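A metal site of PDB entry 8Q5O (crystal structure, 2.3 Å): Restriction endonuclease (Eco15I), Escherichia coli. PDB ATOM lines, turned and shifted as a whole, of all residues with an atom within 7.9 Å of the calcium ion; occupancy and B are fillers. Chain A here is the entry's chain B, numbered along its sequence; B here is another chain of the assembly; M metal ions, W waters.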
ATOM      1  N   GLY A  40      -4.891   9.935  23.005  1.00  0.00           N
ATOM      2  CA  GLY A  40      -4.597   9.593  21.602  1.00  0.00           C
ATOM      3  C   GLY A  40      -3.117   9.648  21.285  1.00  0.00           C
ATOM      4  O   GLY A  40      -2.619   8.710  20.646  1.00  0.00           O
ATOM      5  N   ASP A  41      -2.465  10.716  21.718  1.00  0.00           N
ATOM      6  CA  ASP A  41      -1.039  10.862  21.401  1.00  0.00           C
ATOM      7  C   ASP A  41      -0.233   9.962  22.320  1.00  0.00           C
ATOM      8  O   ASP A  41       0.823   9.476  21.924  1.00  0.00           O
ATOM      9  CB  ASP A  41      -0.555  12.295  21.507  1.00  0.00           C
ATOM     10  CG  ASP A  41      -0.958  13.146  20.338  1.00  0.00           C
ATOM     11  OD1 ASP A  41      -1.237  12.615  19.230  1.00  0.00           O
ATOM     12  OD2 ASP A  41      -1.030  14.356  20.555  1.00  0.00           O
ATOM     13  N   ALA A  43      -1.348   7.054  23.281  1.00  0.00           N
ATOM     14  CA  ALA A  43      -1.503   5.777  22.596  1.00  0.00           C
ATOM     15  C   ALA A  43      -0.506   5.701  21.432  1.00  0.00           C
ATOM     16  O   ALA A  43       0.306   4.787  21.391  1.00  0.00           O
ATOM     17  CB  ALA A  43      -2.966   5.571  22.173  1.00  0.00           C
ATOM     18  N   GLU A  44      -0.599   6.638  20.487  1.00  0.00           N
ATOM     19  CA  GLU A  44       0.366   6.747  19.388  1.00  0.00           C
ATOM     20  C   GLU A  44       1.801   6.615  19.888  1.00  0.00           C
ATOM     21  O   GLU A  44       2.587   5.877  19.281  1.00  0.00           O
ATOM     22  CB  GLU A  44       0.246   8.091  18.634  1.00  0.00           C
ATOM     23  CG  GLU A  44      -0.724   8.058  17.462  1.00  0.00           C
ATOM     24  CD  GLU A  44      -1.634   9.275  17.328  1.00  0.00           C
ATOM     25  OE1 GLU A  44      -1.899   9.968  18.349  1.00  0.00           O
ATOM     26  OE2 GLU A  44      -2.090   9.510  16.198  1.00  0.00           O
ATOM     27  N   SER A  59      -0.541  13.362  10.000  1.00  0.00           N
ATOM     28  CA  SER A  59      -1.559  12.334  10.192  1.00  0.00           C
ATOM     29  C   SER A  59      -2.709  12.578   9.216  1.00  0.00           C
ATOM     30  O   SER A  59      -3.847  12.622   9.647  1.00  0.00           O
ATOM     31  CB  SER A  59      -2.045  12.323  11.621  1.00  0.00           C
ATOM     32  OG  SER A  59      -2.812  11.182  11.887  1.00  0.00           O
ATOM     33  N   GLY A  62      -4.695   9.260   6.859  1.00  0.00           N
ATOM     34  CA  GLY A  62      -5.523   8.300   7.613  1.00  0.00           C
ATOM     35  C   GLY A  62      -4.592   7.318   8.281  1.00  0.00           C
ATOM     36  O   GLY A  62      -5.081   6.415   8.964  1.00  0.00           O
ATOM     37  N   ALA A  63      -3.289   7.504   8.085  1.00  0.00           N
ATOM     38  CA  ALA A  63      -2.288   6.668   8.775  1.00  0.00           C
ATOM     39  C   ALA A  63      -1.543   7.521   9.808  1.00  0.00           C
ATOM     40  O   ALA A  63      -1.444   8.741   9.609  1.00  0.00           O
ATOM     41  CB  ALA A  63      -1.352   6.055   7.764  1.00  0.00           C
ATOM     42  N   ASP A  64      -1.076   6.888  10.885  1.00  0.00           N
ATOM     43  CA  ASP A  64      -0.408   7.637  11.972  1.00  0.00           C
ATOM     44  C   ASP A  64       1.039   7.153  12.151  1.00  0.00           C
ATOM     45  O   ASP A  64       1.771   7.817  12.877  1.00  0.00           O
ATOM     46  CB  ASP A  64      -1.199   7.526  13.281  1.00  0.00           C
ATOM     47  CG  ASP A  64      -2.622   8.065  13.201  1.00  0.00           C
ATOM     48  OD1 ASP A  64      -3.008   8.522  12.109  1.00  0.00           O
ATOM     49  OD2 ASP A  64      -3.317   8.019  14.225  1.00  0.00           O
ATOM     50  N   VAL A  73      -0.033   2.346   9.247  1.00  0.00           N
ATOM     51  CA  VAL A  73      -0.893   1.946  10.390  1.00  0.00           C
ATOM     52  C   VAL A  73      -1.684   3.143  10.918  1.00  0.00           C
ATOM     53  O   VAL A  73      -1.049   4.166  11.206  1.00  0.00           O
ATOM     54  CB  VAL A  73      -0.060   1.312  11.516  1.00  0.00           C
ATOM     55  CG1 VAL A  73      -0.877   1.115  12.783  1.00  0.00           C
ATOM     56  CG2 VAL A  73       0.576   0.007  11.080  1.00  0.00           C
ATOM     57  N   GLN A  74      -3.004   3.016  11.032  1.00  0.00           N
ATOM     58  CA  GLN A  74      -3.823   4.078  11.668  1.00  0.00           C
ATOM     59  C   GLN A  74      -3.928   3.752  13.168  1.00  0.00           C
ATOM     60  O   GLN A  74      -4.202   2.598  13.493  1.00  0.00           O
ATOM     61  CB  GLN A  74      -5.212   4.180  11.034  1.00  0.00           C
ATOM     62  CG  GLN A  74      -6.179   5.035  11.832  1.00  0.00           C
ATOM     63  CD  GLN A  74      -5.612   6.374  12.236  1.00  0.00           C
ATOM     64  OE1 GLN A  74      -5.525   6.690  13.421  1.00  0.00           O
ATOM     65  NE2 GLN A  74      -5.242   7.173  11.259  1.00  0.00           N
ATOM     66  N   ILE A  75      -3.676   4.733  14.035  1.00  0.00           N
ATOM     67  CA  ILE A  75      -3.654   4.458  15.494  1.00  0.00           C
ATOM     68  C   ILE A  75      -4.813   5.240  16.128  1.00  0.00           C
ATOM     69  O   ILE A  75      -4.824   6.481  16.028  1.00  0.00           O
ATOM     70  CB  ILE A  75      -2.295   4.847  16.105  1.00  0.00           C
ATOM     71  CG1 ILE A  75      -1.152   4.001  15.536  1.00  0.00           C
ATOM     72  CG2 ILE A  75      -2.347   4.772  17.616  1.00  0.00           C
ATOM     73  CD1 ILE A  75      -1.136   2.583  16.029  1.00  0.00           C
ATOM     74  N   LYS A  76      -5.737   4.520  16.756  1.00  0.00           N
ATOM     75  CA  LYS A  76      -6.923   5.174  17.370  1.00  0.00           C
ATOM     76  C   LYS A  76      -7.133   4.547  18.760  1.00  0.00           C
ATOM     77  O   LYS A  76      -7.165   3.312  18.859  1.00  0.00           O
ATOM     78  CB  LYS A  76      -8.113   5.027  16.421  1.00  0.00           C
ATOM     79  CG  LYS A  76      -8.108   5.982  15.236  1.00  0.00           C
ATOM     80  CD  LYS A  76      -9.463   6.147  14.592  1.00  0.00           C
ATOM     81  CE  LYS A  76      -9.575   7.379  13.736  1.00  0.00           C
ATOM     82  NZ  LYS A  76      -8.633   7.345  12.587  1.00  0.00           N
ATOM     83  N   SER A  90     -12.982   6.812  16.564  1.00  0.00           N
ATOM     84  CA  SER A  90     -12.990   8.080  15.886  1.00  0.00           C
ATOM     85  C   SER A  90     -13.313   7.880  14.407  1.00  0.00           C
ATOM     86  O   SER A  90     -13.219   6.762  13.869  1.00  0.00           O
ATOM     87  CB  SER A  90     -11.666   8.784  16.080  1.00  0.00           C
ATOM     88  OG  SER A  90     -11.815  10.185  15.903  1.00  0.00           O
ATOM     89  N   ALA A  91     -13.691   8.968  13.754  1.00  0.00           N
ATOM     90  CA  ALA A  91     -14.053   8.940  12.339  1.00  0.00           C
ATOM     91  C   ALA A  91     -12.881   8.476  11.466  1.00  0.00           C
ATOM     92  O   ALA A  91     -11.742   8.969  11.615  1.00  0.00           O
ATOM     93  CB  ALA A  91     -14.517  10.325  11.909  1.00  0.00           C
ATOM     94  N   LEU A  92     -13.163   7.547  10.555  1.00  0.00           N
ATOM     95  CA  LEU A  92     -12.298   7.281   9.414  1.00  0.00           C
ATOM     96  C   LEU A  92     -12.809   8.087   8.213  1.00  0.00           C
ATOM     97  O   LEU A  92     -13.238   7.543   7.191  1.00  0.00           O
ATOM     98  CB  LEU A  92     -12.273   5.764   9.162  1.00  0.00           C
ATOM     99  CG  LEU A  92     -11.020   5.067   9.688  1.00  0.00           C
ATOM    100  CD1 LEU A  92     -10.850   5.305  11.166  1.00  0.00           C
ATOM    101  CD2 LEU A  92     -11.066   3.604   9.414  1.00  0.00           C
ATOM    102  N   LEU A 103      -5.322  -1.493  11.085  1.00  0.00           N
ATOM    103  CA  LEU A 103      -5.621  -0.503  12.106  1.00  0.00           C
ATOM    104  C   LEU A 103      -5.376  -1.113  13.473  1.00  0.00           C
ATOM    105  O   LEU A 103      -5.629  -2.286  13.678  1.00  0.00           O
ATOM    106  CB  LEU A 103      -7.064  -0.024  11.950  1.00  0.00           C
ATOM    107  CG  LEU A 103      -7.388   1.339  12.562  1.00  0.00           C
ATOM    108  CD1 LEU A 103      -8.458   2.021  11.726  1.00  0.00           C
ATOM    109  CD2 LEU A 103      -7.831   1.199  14.024  1.00  0.00           C
ATOM    110  N   ILE A 104      -4.857  -0.284  14.403  1.00  0.00           N
ATOM    111  CA  ILE A 104      -4.664  -0.709  15.780  1.00  0.00           C
ATOM    112  C   ILE A 104      -5.494   0.215  16.686  1.00  0.00           C
ATOM    113  O   ILE A 104      -5.290   1.434  16.715  1.00  0.00           O
ATOM    114  CB  ILE A 104      -3.170  -0.729  16.160  1.00  0.00           C
ATOM    115  CG1 ILE A 104      -2.496  -1.985  15.615  1.00  0.00           C
ATOM    116  CG2 ILE A 104      -2.993  -0.626  17.669  1.00  0.00           C
ATOM    117  CD1 ILE A 104      -1.111  -2.211  16.181  1.00  0.00           C
ATOM    118  N1  5CM B   4      -8.235  16.300  13.188  1.00  0.00           N
ATOM    119  C2  5CM B   4      -8.625  16.918  14.367  1.00  0.00           C
ATOM    120  N3  5CM B   4      -9.888  17.402  14.464  1.00  0.00           N
ATOM    121  C4  5CM B   4     -10.720  17.306  13.425  1.00  0.00           C
ATOM    122  C5  5CM B   4     -10.332  16.702  12.210  1.00  0.00           C
ATOM    123  C5A 5CM B   4     -11.289  16.604  11.061  1.00  0.00           C
ATOM    124  C6  5CM B   4      -9.085  16.216  12.128  1.00  0.00           C
ATOM    125  O2  5CM B   4      -7.826  16.977  15.312  1.00  0.00           O
ATOM    126  N4  5CM B   4     -11.947  17.819  13.593  1.00  0.00           N
ATOM    127  C1' 5CM B   4      -6.852  15.772  13.074  1.00  0.00           C
ATOM    128  C2' 5CM B   4      -6.568  14.557  13.930  1.00  0.00           C
ATOM    129  C3' 5CM B   4      -6.452  13.411  12.926  1.00  0.00           C
ATOM    130  C4' 5CM B   4      -6.034  14.126  11.650  1.00  0.00           C
ATOM    131  O4' 5CM B   4      -6.645  15.429  11.721  1.00  0.00           O
ATOM    132  O3' 5CM B   4      -5.433  12.498  13.318  1.00  0.00           O
ATOM    133  C5' 5CM B   4      -6.451  13.413  10.384  1.00  0.00           C
ATOM    134  O5' 5CM B   4      -7.486  14.161   9.703  1.00  0.00           O
ATOM    135  P   5CM B   4      -7.915  13.678   8.243  1.00  0.00           P
ATOM    136  OP1 5CM B   4      -7.495  12.233   8.100  1.00  0.00           O
ATOM    137  OP2 5CM B   4      -9.383  13.915   8.086  1.00  0.00           O
ATOM    138  P    DT B   5      -6.163  11.119  13.676  1.00  0.00           P
ATOM    139  OP1  DT B   5      -5.198   9.958  13.764  1.00  0.00           O
ATOM    140  OP2  DT B   5      -7.352  10.876  12.788  1.00  0.00           O
ATOM    141  O5'  DT B   5      -6.705  11.403  15.153  1.00  0.00           O
ATOM    142  C5'  DT B   5      -5.737  11.594  16.212  1.00  0.00           C
ATOM    143  C4'  DT B   5      -6.420  12.140  17.440  1.00  0.00           C
ATOM    144  O4'  DT B   5      -7.140  13.346  17.126  1.00  0.00           O
ATOM    145  C3'  DT B   5      -7.467  11.242  18.077  1.00  0.00           C
ATOM    146  O3'  DT B   5      -6.839  10.283  18.917  1.00  0.00           O
ATOM    147  C2'  DT B   5      -8.263  12.239  18.891  1.00  0.00           C
ATOM    148  C1'  DT B   5      -8.134  13.554  18.114  1.00  0.00           C
ATOM    149  N1   DT B   5      -9.372  13.974  17.439  1.00  0.00           N
ATOM    150  C2   DT B   5     -10.278  14.736  18.156  1.00  0.00           C
ATOM    151  O2   DT B   5     -10.093  15.061  19.317  1.00  0.00           O
ATOM    152  N3   DT B   5     -11.410  15.079  17.474  1.00  0.00           N
ATOM    153  C4   DT B   5     -11.728  14.752  16.167  1.00  0.00           C
ATOM    154  O4   DT B   5     -12.790  15.146  15.686  1.00  0.00           O
ATOM    155  C5   DT B   5     -10.739  13.960  15.475  1.00  0.00           C
ATOM    156  C7   DT B   5     -10.992  13.566  14.054  1.00  0.00           C
ATOM    157  C6   DT B   5      -9.625  13.612  16.142  1.00  0.00           C
ATOM    158  P    DG B   6      -7.747   8.974  19.124  1.00  0.00           P
ATOM    159  OP1  DG B   6      -6.917   7.855  19.700  1.00  0.00           O
ATOM    160  OP2  DG B   6      -8.505   8.601  17.882  1.00  0.00           O
ATOM    161  O5'  DG B   6      -8.815   9.403  20.236  1.00  0.00           O
ATOM    162  C5'  DG B   6      -8.348   9.823  21.535  1.00  0.00           C
ATOM    163  C4'  DG B   6      -9.385  10.699  22.188  1.00  0.00           C
ATOM    164  O4'  DG B   6      -9.994  11.533  21.182  1.00  0.00           O
ATOM    165  C3'  DG B   6     -10.515   9.947  22.897  1.00  0.00           C
ATOM    166  O3'  DG B   6     -10.639  10.417  24.234  1.00  0.00           O
ATOM    167  C2'  DG B   6     -11.756  10.289  22.091  1.00  0.00           C
ATOM    168  C1'  DG B   6     -11.393  11.590  21.417  1.00  0.00           C
ATOM    169  N9   DG B   6     -12.050  11.771  20.130  1.00  0.00           N
ATOM    170  C8   DG B   6     -11.686  11.268  18.908  1.00  0.00           C
ATOM    171  N7   DG B   6     -12.513  11.591  17.948  1.00  0.00           N
ATOM    172  C5   DG B   6     -13.498  12.340  18.582  1.00  0.00           C
ATOM    173  C6   DG B   6     -14.660  12.951  18.055  1.00  0.00           C
ATOM    174  O6   DG B   6     -15.057  12.952  16.881  1.00  0.00           O
ATOM    175  N1   DG B   6     -15.386  13.604  19.045  1.00  0.00           N
ATOM    176  C2   DG B   6     -15.040  13.666  20.377  1.00  0.00           C
ATOM    177  N2   DG B   6     -15.850  14.352  21.183  1.00  0.00           N
ATOM    178  N3   DG B   6     -13.945  13.093  20.869  1.00  0.00           N
ATOM    179  C4   DG B   6     -13.226  12.447  19.920  1.00  0.00           C
HETATM  180 CA    CA M   1      -5.247   8.415  15.308  1.00  0.00          CA
HETATM  181  O   HOH W   1      -7.681   8.955  15.016  1.00  0.00           O
HETATM  182  O   HOH W   2      -4.824   8.742  18.026  1.00  0.00           O
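The side-chain amide oxygen of Gln 74 sits close to the side-chain amino group of Lys 76, 3.3 Å away. The backbone NH (N) of Ile 104 is in hydrogen-bond range of the backbone carbonyl oxygen (O) of Gln 74 (3.1 Å). The side-chain amide nitrogen of Gln 74 is in hydrogen-bond range of the backbone carbonyl oxygen of Gly 62, 2.4 Å away. The backbone NH of Asp 41 sits close to the side-chain carboxylate of Glu 44 (3.5 Å). The backbone carbonyl oxygen (O) of Ile 104 sits at hydrogen-bond distance from the backbone NH (N) of Lys 76 (3.1 Å). N of Asp 64 lies within hydrogen-bond range of O of Val 73. OP1 of DT 5 of chain B lies close to OG of Ser 59 (3.3 Å). OP2 of DT 5 of chain B is in salt-bridge range of the side-chain amino group of Lys 76, 3.8 Å away.
Glu 44 touches the calcium ion (OE2 to CA, 3.5 Å). Lys 76 touches the calcium ion (CG to CA, 3.8 Å). Six residues have an atom within 4 Å of the calcium ion: Glu 44, Asp 64, Gln 74, Ile 75, Lys 76 and DT 5 of chain B.
The calcium ion is bound by the backbone carbonyl oxygen (O) of Ile 75 (2.1 Å), OP1 of DT 5 of chain B (2.2 Å), the side-chain carboxylate (OD2) of Asp 64 (2.2 Å), water W1 (2.5 Å), the side-chain amide oxygen (OE1) of Gln 74 (2.6 Å) and water W2 (2.8 Å). The calcium ion has six donor atoms within binding distance.
Water W1 lies within hydrogen-bond range of O5' of DT 5 of chain B, OP2 of DG 6 of chain B and NZ of Lys 76.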
